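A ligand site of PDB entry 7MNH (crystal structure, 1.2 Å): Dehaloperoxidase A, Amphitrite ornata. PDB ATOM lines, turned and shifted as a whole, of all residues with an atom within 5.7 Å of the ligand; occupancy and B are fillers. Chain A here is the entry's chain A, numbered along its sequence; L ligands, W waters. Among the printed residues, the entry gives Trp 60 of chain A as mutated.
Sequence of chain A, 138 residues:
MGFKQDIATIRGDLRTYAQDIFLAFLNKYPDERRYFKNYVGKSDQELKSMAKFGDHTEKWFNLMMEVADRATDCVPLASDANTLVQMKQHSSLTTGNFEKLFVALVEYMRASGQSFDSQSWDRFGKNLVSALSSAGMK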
ATOM      1  N   PHE A  25     -19.693 -25.732  -1.905  1.00  0.00           N
ATOM      2  CA  PHE A  25     -20.358 -26.958  -1.397  1.00  0.00           C
ATOM      3  C   PHE A  25     -20.874 -27.798  -2.551  1.00  0.00           C
ATOM      4  O   PHE A  25     -20.573 -29.015  -2.637  1.00  0.00           O
ATOM      5  CB  PHE A  25     -21.431 -26.526  -0.401  1.00  0.00           C
ATOM      6  CG  PHE A  25     -22.405 -27.579  -0.023  1.00  0.00           C
ATOM      7  CD1 PHE A  25     -22.003 -28.796   0.546  1.00  0.00           C
ATOM      8  CD2 PHE A  25     -23.748 -27.375  -0.214  1.00  0.00           C
ATOM      9  CE1 PHE A  25     -22.922 -29.757   0.927  1.00  0.00           C
ATOM     10  CE2 PHE A  25     -24.674 -28.327   0.198  1.00  0.00           C
ATOM     11  CZ  PHE A  25     -24.243 -29.531   0.738  1.00  0.00           C
ATOM     12  N   GLU A  32     -25.396 -33.075  -4.149  1.00  0.00           N
ATOM     13  CA  GLU A  32     -26.221 -32.280  -3.199  1.00  0.00           C
ATOM     14  C   GLU A  32     -27.150 -31.289  -3.927  1.00  0.00           C
ATOM     15  O   GLU A  32     -28.089 -30.816  -3.336  1.00  0.00           O
ATOM     16  CB  GLU A  32     -25.316 -31.539  -2.222  1.00  0.00           C
ATOM     17  CG  GLU A  32     -24.508 -32.442  -1.304  1.00  0.00           C
ATOM     18  CD  GLU A  32     -25.323 -33.260  -0.339  1.00  0.00           C
ATOM     19  OE1 GLU A  32     -25.964 -32.665   0.495  1.00  0.00           O
ATOM     20  OE2 GLU A  32     -25.361 -34.527  -0.515  1.00  0.00           O
ATOM     21  N   TYR A  35     -31.206 -31.484  -4.036  1.00  0.00           N
ATOM     22  CA  TYR A  35     -32.142 -30.886  -3.045  1.00  0.00           C
ATOM     23  C   TYR A  35     -32.613 -29.508  -3.437  1.00  0.00           C
ATOM     24  O   TYR A  35     -33.528 -28.996  -2.807  1.00  0.00           O
ATOM     25  CB  TYR A  35     -31.445 -30.817  -1.697  1.00  0.00           C
ATOM     26  CG  TYR A  35     -31.120 -32.148  -1.109  1.00  0.00           C
ATOM     27  CD1 TYR A  35     -32.109 -32.986  -0.588  1.00  0.00           C
ATOM     28  CD2 TYR A  35     -29.822 -32.598  -1.095  1.00  0.00           C
ATOM     29  CE1 TYR A  35     -31.779 -34.196  -0.013  1.00  0.00           C
ATOM     30  CE2 TYR A  35     -29.496 -33.835  -0.593  1.00  0.00           C
ATOM     31  CZ  TYR A  35     -30.473 -34.605  -0.015  1.00  0.00           C
ATOM     32  OH  TYR A  35     -30.081 -35.810   0.491  1.00  0.00           O
ATOM     33  N   PHE A  36     -32.110 -28.959  -4.512  1.00  0.00           N
ATOM     34  CA  PHE A  36     -32.401 -27.600  -4.998  1.00  0.00           C
ATOM     35  C   PHE A  36     -32.822 -27.735  -6.448  1.00  0.00           C
ATOM     36  O   PHE A  36     -32.068 -27.412  -7.350  1.00  0.00           O
ATOM     37  CB  PHE A  36     -31.156 -26.726  -4.833  1.00  0.00           C
ATOM     38  CG  PHE A  36     -30.584 -26.734  -3.444  1.00  0.00           C
ATOM     39  CD1 PHE A  36     -31.053 -25.856  -2.497  1.00  0.00           C
ATOM     40  CD2 PHE A  36     -29.599 -27.629  -3.104  1.00  0.00           C
ATOM     41  CE1 PHE A  36     -30.517 -25.861  -1.207  1.00  0.00           C
ATOM     42  CE2 PHE A  36     -29.052 -27.644  -1.832  1.00  0.00           C
ATOM     43  CZ  PHE A  36     -29.531 -26.756  -0.889  1.00  0.00           C
ATOM     44  N   TYR A  39     -32.124 -25.223  -9.218  1.00  0.00           N
ATOM     45  CA  TYR A  39     -30.724 -24.846  -9.557  1.00  0.00           C
ATOM     46  C   TYR A  39     -30.087 -25.837 -10.532  1.00  0.00           C
ATOM     47  O   TYR A  39     -28.954 -25.607 -10.962  1.00  0.00           O
ATOM     48  CB  TYR A  39     -29.877 -24.718  -8.293  1.00  0.00           C
ATOM     49  CG  TYR A  39     -30.373 -23.733  -7.262  1.00  0.00           C
ATOM     50  CD1 TYR A  39     -31.311 -22.750  -7.503  1.00  0.00           C
ATOM     51  CD2 TYR A  39     -29.889 -23.871  -5.976  1.00  0.00           C
ATOM     52  CE1 TYR A  39     -31.774 -21.924  -6.485  1.00  0.00           C
ATOM     53  CE2 TYR A  39     -30.342 -23.065  -4.955  1.00  0.00           C
ATOM     54  CZ  TYR A  39     -31.278 -22.111  -5.219  1.00  0.00           C
ATOM     55  OH  TYR A  39     -31.661 -21.292  -4.180  1.00  0.00           O
ATOM     56  N   ASP A  55     -31.514 -14.792  -2.374  1.00  0.00           N
ATOM     57  CA  ASP A  55     -32.326 -14.558  -1.163  1.00  0.00           C
ATOM     58  C   ASP A  55     -32.251 -15.770  -0.238  1.00  0.00           C
ATOM     59  O   ASP A  55     -31.991 -15.574   0.987  1.00  0.00           O
ATOM     60  CB  ASP A  55     -33.758 -14.209  -1.569  1.00  0.00           C
ATOM     61  CG  ASP A  55     -34.603 -13.733  -0.408  1.00  0.00           C
ATOM     62  OD1 ASP A  55     -34.369 -12.610   0.076  1.00  0.00           O
ATOM     63  OD2 ASP A  55     -35.442 -14.492   0.006  1.00  0.00           O
ATOM     64  N   HIS A  56     -32.459 -16.951  -0.746  1.00  0.00           N
ATOM     65  CA  HIS A  56     -32.481 -18.126   0.127  1.00  0.00           C
ATOM     66  C   HIS A  56     -31.096 -18.419   0.612  1.00  0.00           C
ATOM     67  O   HIS A  56     -30.936 -18.757   1.808  1.00  0.00           O
ATOM     68  CB  HIS A  56     -33.136 -19.307  -0.586  1.00  0.00           C
ATOM     69  CG  HIS A  56     -34.615 -19.078  -0.760  1.00  0.00           C
ATOM     70  ND1 HIS A  56     -35.472 -20.069  -1.162  1.00  0.00           N
ATOM     71  CD2 HIS A  56     -35.359 -17.938  -0.699  1.00  0.00           C
ATOM     72  CE1 HIS A  56     -36.683 -19.583  -1.229  1.00  0.00           C
ATOM     73  NE2 HIS A  56     -36.675 -18.289  -1.000  1.00  0.00           N
ATOM     74  N   THR A  57     -30.081 -18.240  -0.197  1.00  0.00           N
ATOM     75  CA  THR A  57     -28.746 -18.585   0.258  1.00  0.00           C
ATOM     76  C   THR A  57     -28.290 -17.574   1.308  1.00  0.00           C
ATOM     77  O   THR A  57     -27.693 -17.977   2.321  1.00  0.00           O
ATOM     78  CB  THR A  57     -27.852 -18.716  -0.959  1.00  0.00           C
ATOM     79  OG1 THR A  57     -28.468 -19.618  -1.874  1.00  0.00           O
ATOM     80  CG2 THR A  57     -26.484 -19.198  -0.540  1.00  0.00           C
ATOM     81  N   LYS A  59     -30.265 -15.993   3.357  1.00  0.00           N
ATOM     82  CA  LYS A  59     -31.029 -16.258   4.601  1.00  0.00           C
ATOM     83  C   LYS A  59     -30.503 -17.485   5.318  1.00  0.00           C
ATOM     84  O   LYS A  59     -30.479 -17.509   6.560  1.00  0.00           O
ATOM     85  CB  LYS A  59     -32.501 -16.354   4.262  1.00  0.00           C
ATOM     86  CG  LYS A  59     -33.070 -14.962   3.942  1.00  0.00           C
ATOM     87  CD  LYS A  59     -34.502 -14.899   3.405  1.00  0.00           C
ATOM     88  CE  LYS A  59     -34.878 -13.458   3.026  1.00  0.00           C
ATOM     89  NZ  LYS A  59     -36.180 -13.444   2.341  1.00  0.00           N
ATOM     90  N   TRP A  60     -30.063 -18.521   4.529  1.00  0.00           N
ATOM     91  CA  TRP A  60     -29.362 -19.697   5.119  1.00  0.00           C
ATOM     92  C   TRP A  60     -28.215 -19.162   5.978  1.00  0.00           C
ATOM     93  O   TRP A  60     -28.162 -19.444   7.198  1.00  0.00           O
ATOM     94  CB  TRP A  60     -28.730 -20.522   4.002  1.00  0.00           C
ATOM     95  CG  TRP A  60     -29.051 -21.935   3.682  1.00  0.00           C
ATOM     96  CD1 TRP A  60     -30.268 -22.506   3.458  1.00  0.00           C
ATOM     97  CD2 TRP A  60     -28.066 -22.903   3.249  1.00  0.00           C
ATOM     98  NE1 TRP A  60     -30.099 -23.819   3.120  1.00  0.00           N
ATOM     99  CE2 TRP A  60     -28.763 -24.069   2.915  1.00  0.00           C
ATOM    100  CE3 TRP A  60     -26.666 -22.917   3.230  1.00  0.00           C
ATOM    101  CZ2 TRP A  60     -28.110 -25.219   2.468  1.00  0.00           C
ATOM    102  CZ3 TRP A  60     -26.020 -24.048   2.792  1.00  0.00           C
ATOM    103  CH2 TRP A  60     -26.738 -25.184   2.414  1.00  0.00           C
ATOM    104  N   PHE A  61     -27.281 -18.470   5.315  1.00  0.00           N
ATOM    105  CA  PHE A  61     -26.042 -18.075   5.976  1.00  0.00           C
ATOM    106  C   PHE A  61     -26.300 -17.074   7.073  1.00  0.00           C
ATOM    107  O   PHE A  61     -25.534 -17.039   8.057  1.00  0.00           O
ATOM    108  CB  PHE A  61     -24.998 -17.598   4.983  1.00  0.00           C
ATOM    109  CG  PHE A  61     -24.330 -18.789   4.324  1.00  0.00           C
ATOM    110  CD1 PHE A  61     -24.962 -19.530   3.352  1.00  0.00           C
ATOM    111  CD2 PHE A  61     -23.101 -19.209   4.807  1.00  0.00           C
ATOM    112  CE1 PHE A  61     -24.301 -20.625   2.786  1.00  0.00           C
ATOM    113  CE2 PHE A  61     -22.450 -20.285   4.237  1.00  0.00           C
ATOM    114  CZ  PHE A  61     -23.060 -20.994   3.244  1.00  0.00           C
ATOM    115  N   LEU A  63     -28.861 -17.219   9.140  1.00  0.00           N
ATOM    116  CA  LEU A  63     -29.173 -18.074  10.293  1.00  0.00           C
ATOM    117  C   LEU A  63     -27.911 -18.783  10.766  1.00  0.00           C
ATOM    118  O   LEU A  63     -27.701 -18.949  11.988  1.00  0.00           O
ATOM    119  CB  LEU A  63     -30.298 -19.037   9.938  1.00  0.00           C
ATOM    120  CG  LEU A  63     -30.682 -19.994  11.079  1.00  0.00           C
ATOM    121  CD1 LEU A  63     -31.082 -19.214  12.335  1.00  0.00           C
ATOM    122  CD2 LEU A  63     -31.822 -20.925  10.648  1.00  0.00           C
ATOM    123  N   MET A  64     -27.064 -19.247   9.848  1.00  0.00           N
ATOM    124  CA  MET A  64     -25.812 -19.885  10.296  1.00  0.00           C
ATOM    125  C   MET A  64     -25.032 -18.915  11.181  1.00  0.00           C
ATOM    126  O   MET A  64     -24.452 -19.360  12.205  1.00  0.00           O
ATOM    127  CB  MET A  64     -24.958 -20.299   9.098  1.00  0.00           C
ATOM    128  CG  MET A  64     -23.830 -21.182   9.531  1.00  0.00           C
ATOM    129  SD  MET A  64     -22.586 -21.518   8.269  1.00  0.00           S
ATOM    130  CE  MET A  64     -23.532 -22.474   7.108  1.00  0.00           C
ATOM    131  N   VAL A  67     -26.567 -18.641  14.653  1.00  0.00           N
ATOM    132  CA  VAL A  67     -26.262 -19.850  15.455  1.00  0.00           C
ATOM    133  C   VAL A  67     -24.808 -19.769  15.909  1.00  0.00           C
ATOM    134  O   VAL A  67     -24.476 -20.039  17.080  1.00  0.00           O
ATOM    135  CB  VAL A  67     -26.551 -21.113  14.645  1.00  0.00           C
ATOM    136  CG1 VAL A  67     -26.111 -22.345  15.394  1.00  0.00           C
ATOM    137  CG2 VAL A  67     -28.027 -21.209  14.315  1.00  0.00           C
ATOM    138  N   LEU A  84     -33.166 -26.117  13.208  1.00  0.00           N
ATOM    139  CA  LEU A  84     -32.662 -26.622  11.923  1.00  0.00           C
ATOM    140  C   LEU A  84     -33.268 -27.996  11.617  1.00  0.00           C
ATOM    141  O   LEU A  84     -33.553 -28.296  10.463  1.00  0.00           O
ATOM    142  CB  LEU A  84     -31.134 -26.674  11.963  1.00  0.00           C
ATOM    143  CG  LEU A  84     -30.403 -25.335  12.027  1.00  0.00           C
ATOM    144  CD1 LEU A  84     -28.918 -25.576  12.250  1.00  0.00           C
ATOM    145  CD2 LEU A  84     -30.714 -24.502  10.798  1.00  0.00           C
ATOM    146  N   MET A  87     -37.215 -27.566  10.664  1.00  0.00           N
ATOM    147  CA  MET A  87     -37.606 -26.776   9.457  1.00  0.00           C
ATOM    148  C   MET A  87     -38.140 -27.720   8.378  1.00  0.00           C
ATOM    149  O   MET A  87     -37.491 -28.683   8.032  1.00  0.00           O
ATOM    150  CB  MET A  87     -36.394 -26.057   8.870  1.00  0.00           C
ATOM    151  CG  MET A  87     -36.084 -24.810   9.623  1.00  0.00           C
ATOM    152  SD  MET A  87     -34.515 -24.101   9.156  1.00  0.00           S
ATOM    153  CE  MET A  87     -34.713 -23.874   7.381  1.00  0.00           C
ATOM    154  N   GLN A  89     -38.212 -27.340   5.293  1.00  0.00           N
ATOM    155  CA  GLN A  89     -37.268 -27.352   4.146  1.00  0.00           C
ATOM    156  C   GLN A  89     -36.135 -28.337   4.369  1.00  0.00           C
ATOM    157  O   GLN A  89     -35.415 -28.615   3.425  1.00  0.00           O
ATOM    158  CB  GLN A  89     -36.671 -25.967   3.896  1.00  0.00           C
ATOM    159  CG  GLN A  89     -37.715 -24.917   3.635  1.00  0.00           C
ATOM    160  CD  GLN A  89     -37.924 -24.121   4.919  1.00  0.00           C
ATOM    161  OE1 GLN A  89     -38.198 -24.633   6.033  1.00  0.00           O
ATOM    162  NE2 GLN A  89     -37.685 -22.843   4.737  1.00  0.00           N
ATOM    163  N   HIS A  90     -35.920 -28.784   5.612  1.00  0.00           N
ATOM    164  CA  HIS A  90     -34.853 -29.757   5.972  1.00  0.00           C
ATOM    165  C   HIS A  90     -35.396 -31.149   6.228  1.00  0.00           C
ATOM    166  O   HIS A  90     -34.627 -31.977   6.704  1.00  0.00           O
ATOM    167  CB  HIS A  90     -34.069 -29.229   7.190  1.00  0.00           C
ATOM    168  CG  HIS A  90     -33.314 -27.969   6.929  1.00  0.00           C
ATOM    169  ND1 HIS A  90     -32.787 -27.234   7.946  1.00  0.00           N
ATOM    170  CD2 HIS A  90     -32.925 -27.380   5.770  1.00  0.00           C
ATOM    171  CE1 HIS A  90     -32.062 -26.244   7.400  1.00  0.00           C
ATOM    172  NE2 HIS A  90     -32.165 -26.269   6.055  1.00  0.00           N
ATOM    173  N   LEU A  93     -33.323 -34.178   5.012  1.00  0.00           N
ATOM    174  CA  LEU A  93     -31.859 -34.158   5.204  1.00  0.00           C
ATOM    175  C   LEU A  93     -31.468 -35.095   6.334  1.00  0.00           C
ATOM    176  O   LEU A  93     -32.276 -35.468   7.191  1.00  0.00           O
ATOM    177  CB  LEU A  93     -31.422 -32.751   5.543  1.00  0.00           C
ATOM    178  CG  LEU A  93     -31.767 -31.715   4.491  1.00  0.00           C
ATOM    179  CD1 LEU A  93     -31.202 -30.407   4.931  1.00  0.00           C
ATOM    180  CD2 LEU A  93     -31.264 -32.106   3.120  1.00  0.00           C
ATOM    181  N   ASN A  97     -25.531 -34.533   5.270  1.00  0.00           N
ATOM    182  CA  ASN A  97     -25.645 -33.335   4.414  1.00  0.00           C
ATOM    183  C   ASN A  97     -24.911 -32.169   5.090  1.00  0.00           C
ATOM    184  O   ASN A  97     -24.247 -31.397   4.394  1.00  0.00           O
ATOM    185  CB  ASN A  97     -27.083 -32.960   4.122  1.00  0.00           C
ATOM    186  CG  ASN A  97     -27.863 -34.047   3.425  1.00  0.00           C
ATOM    187  OD1 ASN A  97     -28.761 -34.644   3.999  1.00  0.00           O
ATOM    188  ND2 ASN A  97     -27.583 -34.271   2.179  1.00  0.00           N
ATOM    189  N   PHE A  98     -25.067 -32.022   6.401  1.00  0.00           N
ATOM    190  CA  PHE A  98     -24.455 -30.934   7.153  1.00  0.00           C
ATOM    191  C   PHE A  98     -22.962 -31.200   7.264  1.00  0.00           C
ATOM    192  O   PHE A  98     -22.184 -30.215   7.173  1.00  0.00           O
ATOM    193  CB  PHE A  98     -25.138 -30.770   8.524  1.00  0.00           C
ATOM    194  CG  PHE A  98     -26.532 -30.240   8.415  1.00  0.00           C
ATOM    195  CD1 PHE A  98     -27.596 -31.060   8.068  1.00  0.00           C
ATOM    196  CD2 PHE A  98     -26.791 -28.907   8.646  1.00  0.00           C
ATOM    197  CE1 PHE A  98     -28.862 -30.544   7.915  1.00  0.00           C
ATOM    198  CE2 PHE A  98     -28.050 -28.391   8.520  1.00  0.00           C
ATOM    199  CZ  PHE A  98     -29.100 -29.200   8.169  1.00  0.00           C
ATOM    200  N   LEU A 101     -21.481 -30.014   4.042  1.00  0.00           N
ATOM    201  CA  LEU A 101     -21.423 -28.528   4.012  1.00  0.00           C
ATOM    202  C   LEU A 101     -20.222 -27.999   4.798  1.00  0.00           C
ATOM    203  O   LEU A 101     -19.468 -27.130   4.285  1.00  0.00           O
ATOM    204  CB  LEU A 101     -22.730 -27.989   4.584  1.00  0.00           C
ATOM    205  CG  LEU A 101     -22.768 -26.484   4.742  1.00  0.00           C
ATOM    206  CD1 LEU A 101     -22.538 -25.737   3.433  1.00  0.00           C
ATOM    207  CD2 LEU A 101     -24.054 -26.038   5.401  1.00  0.00           C
ATOM    208  N   PHE A 102     -19.994 -28.494   6.000  1.00  0.00           N
ATOM    209  CA  PHE A 102     -18.861 -27.988   6.804  1.00  0.00           C
ATOM    210  C   PHE A 102     -17.531 -28.426   6.228  1.00  0.00           C
ATOM    211  O   PHE A 102     -16.599 -27.592   6.341  1.00  0.00           O
ATOM    212  CB  PHE A 102     -19.057 -28.320   8.283  1.00  0.00           C
ATOM    213  CG  PHE A 102     -20.032 -27.348   8.882  1.00  0.00           C
ATOM    214  CD1 PHE A 102     -19.672 -26.065   9.240  1.00  0.00           C
ATOM    215  CD2 PHE A 102     -21.362 -27.676   9.012  1.00  0.00           C
ATOM    216  CE1 PHE A 102     -20.596 -25.169   9.749  1.00  0.00           C
ATOM    217  CE2 PHE A 102     -22.285 -26.768   9.500  1.00  0.00           C
ATOM    218  CZ  PHE A 102     -21.900 -25.503   9.835  1.00  0.00           C
ATOM    219  N   LEU A 128     -22.144 -28.907  15.886  1.00  0.00           N
ATOM    220  CA  LEU A 128     -23.516 -28.712  15.379  1.00  0.00           C
ATOM    221  C   LEU A 128     -24.079 -30.059  14.915  1.00  0.00           C
ATOM    222  O   LEU A 128     -25.250 -30.345  15.171  1.00  0.00           O
ATOM    223  CB  LEU A 128     -23.540 -27.661  14.267  1.00  0.00           C
ATOM    224  CG  LEU A 128     -24.922 -27.355  13.714  1.00  0.00           C
ATOM    225  CD1 LEU A 128     -25.881 -26.871  14.789  1.00  0.00           C
ATOM    226  CD2 LEU A 128     -24.823 -26.290  12.626  1.00  0.00           C
HETATM  227  C1  LIG L   1     -33.740 -23.579   3.340  1.00  0.00           C
HETATM  228  C2  LIG L   1     -30.716 -22.511   6.985  1.00  0.00           C
HETATM  229  C3  LIG L   1     -28.036 -26.431   5.862  1.00  0.00           C
HETATM  230  C4  LIG L   1     -31.114 -27.454   2.292  1.00  0.00           C
HETATM  231  C5  LIG L   1     -33.137 -22.893   4.407  1.00  0.00           C
HETATM  232  C6  LIG L   1     -33.556 -21.668   4.967  1.00  0.00           C
HETATM  233  C7  LIG L   1     -32.681 -21.380   5.992  1.00  0.00           C
HETATM  234  C8  LIG L   1     -31.747 -22.388   6.080  1.00  0.00           C
HETATM  235  C9  LIG L   1     -32.812 -20.198   6.941  1.00  0.00           C
HETATM  236  C10 LIG L   1     -34.733 -20.846   4.503  1.00  0.00           C
HETATM  237  C11 LIG L   1     -34.379 -19.840   3.371  1.00  0.00           C
HETATM  238  C12 LIG L   1     -35.403 -18.682   3.195  1.00  0.00           C
HETATM  239  O1  LIG L   1     -35.402 -18.094   2.174  1.00  0.00           O
HETATM  240  O2  LIG L   1     -36.154 -18.222   4.064  1.00  0.00           O
HETATM  241  C13 LIG L   1     -29.754 -23.496   7.020  1.00  0.00           C
HETATM  242  C14 LIG L   1     -28.606 -23.473   7.896  1.00  0.00           C
HETATM  243  C15 LIG L   1     -27.812 -24.543   7.603  1.00  0.00           C
HETATM  244  C16 LIG L   1     -28.542 -25.242   6.497  1.00  0.00           C
HETATM  245  C17 LIG L   1     -28.336 -22.406   8.869  1.00  0.00           C
HETATM  246  C18 LIG L   1     -26.590 -25.026   8.180  1.00  0.00           C
HETATM  247  C19 LIG L   1     -26.139 -24.771   9.368  1.00  0.00           C
HETATM  248  C20 LIG L   1     -28.672 -26.996   4.748  1.00  0.00           C
HETATM  249  C21 LIG L   1     -28.109 -28.122   4.091  1.00  0.00           C
HETATM  250  C22 LIG L   1     -28.984 -28.410   3.066  1.00  0.00           C
HETATM  251  C23 LIG L   1     -30.054 -27.522   3.102  1.00  0.00           C
HETATM  252  C24 LIG L   1     -26.850 -28.837   4.447  1.00  0.00           C
HETATM  253  C25 LIG L   1     -28.942 -29.430   1.985  1.00  0.00           C
HETATM  254  C26 LIG L   1     -27.876 -30.079   1.684  1.00  0.00           C
HETATM  255  C27 LIG L   1     -32.107 -26.561   2.292  1.00  0.00           C
HETATM  256  C28 LIG L   1     -33.168 -26.467   1.299  1.00  0.00           C
HETATM  257  C29 LIG L   1     -33.885 -25.393   1.579  1.00  0.00           C
HETATM  258  C30 LIG L   1     -33.260 -24.751   2.771  1.00  0.00           C
HETATM  259  C31 LIG L   1     -33.421 -27.417   0.171  1.00  0.00           C
HETATM  260  C32 LIG L   1     -35.127 -24.906   0.874  1.00  0.00           C
HETATM  261  C33 LIG L   1     -34.894 -24.317  -0.476  1.00  0.00           C
HETATM  262  C34 LIG L   1     -34.094 -23.112  -0.266  1.00  0.00           C
HETATM  263  O3  LIG L   1     -32.925 -23.048  -0.754  1.00  0.00           O
HETATM  264  O4  LIG L   1     -34.555 -22.202   0.400  1.00  0.00           O
HETATM  265  N1  LIG L   1     -32.035 -23.325   5.094  1.00  0.00           N
HETATM  266  N2  LIG L   1     -29.641 -24.553   6.183  1.00  0.00           N
HETATM  267  N3  LIG L   1     -29.795 -26.639   4.161  1.00  0.00           N
HETATM  268  N4  LIG L   1     -32.186 -25.475   3.172  1.00  0.00           N
HETATM  269 FE1  LIG L   1     -31.038 -25.086   4.747  1.00  0.00          FE
HETATM  270  O   HOH W   1     -35.539 -17.522   6.414  1.00  0.00           O
HETATM  271  O   HOH W   2     -30.295 -21.758  -1.452  1.00  0.00           O
HETATM  272  O   HOH W   3     -35.032 -30.328  -0.847  1.00  0.00           O
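A ring nitrogen (ND1) of His 90 sits close to the side-chain sulfur (SD) of Met 87 (3.8 Å).
ND1 of His 90 is in hydrogen-bond range of O of Leu 84, 2.8 Å away.
OH of Tyr 35 lies within hydrogen-bond range of ND2 of Asn 97, at 3.4 Å.
ND2 of Asn 97 lies within hydrogen-bond range of OE1 of Glu 32 (2.8 Å).
OD2 of Asp 55 lies within salt-bridge range of NZ of Lys 59 (2.7 Å).
A ring nitrogen (NE2) of His 90 is bound to an iron atom (FE1) of the ligand (2.1 Å).
An iron atom (FE1) of the ligand is bound by the indole nitrogen (NE1) of Trp 60, at 2.3 Å.
O4 of the ligand sits at hydrogen-bond distance from ND1 of His 56, at 2.8 Å.
Water W2 lies within hydrogen-bond range of OG1 of Thr 57 (2.8 Å), O3 of the ligand (3.0 Å) and OH of Tyr 39 (3.1 Å).
Phe 25 touches the ligand.
Glu 32 touches the ligand (OE1 to C26, 3.4 Å).
Tyr 35 touches the ligand (O to C31, 3.4 Å).
Phe 36 touches the ligand.
CD of Lys 59 touches O1 of the ligand, 3.5 Å away.
CD2 of Leu 63 touches C9 of the ligand, 3.9 Å away.
Met 64 touches the ligand (N to C17, 3.5 Å).
CD2 of Leu 84 touches C17 of the ligand (3.7 Å).
CE of Met 87 touches C6 of the ligand (3.5 Å).
CB of Gln 89 touches C32 of the ligand (3.6 Å).
CD1 of Leu 93 touches C22 of the ligand, 3.5 Å away.
Asn 97 touches the ligand.
CE2 of Phe 98 touches C3 of the ligand, 3.3 Å away.
Leu 101 touches the ligand.
CD2 of Leu 128 touches C19 of the ligand, 3.8 Å away.
Hydrophobic or aromatic side chains that line the ligand: Phe 25, Phe 36, His 56, Trp 60, Leu 63, Met 64, Leu 84, Met 87, His 90, Leu 93, Phe 98, Leu 101 and Leu 128.
The nearest printed residue that does not touch the ligand is Tyr 39 (4.1 Å).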
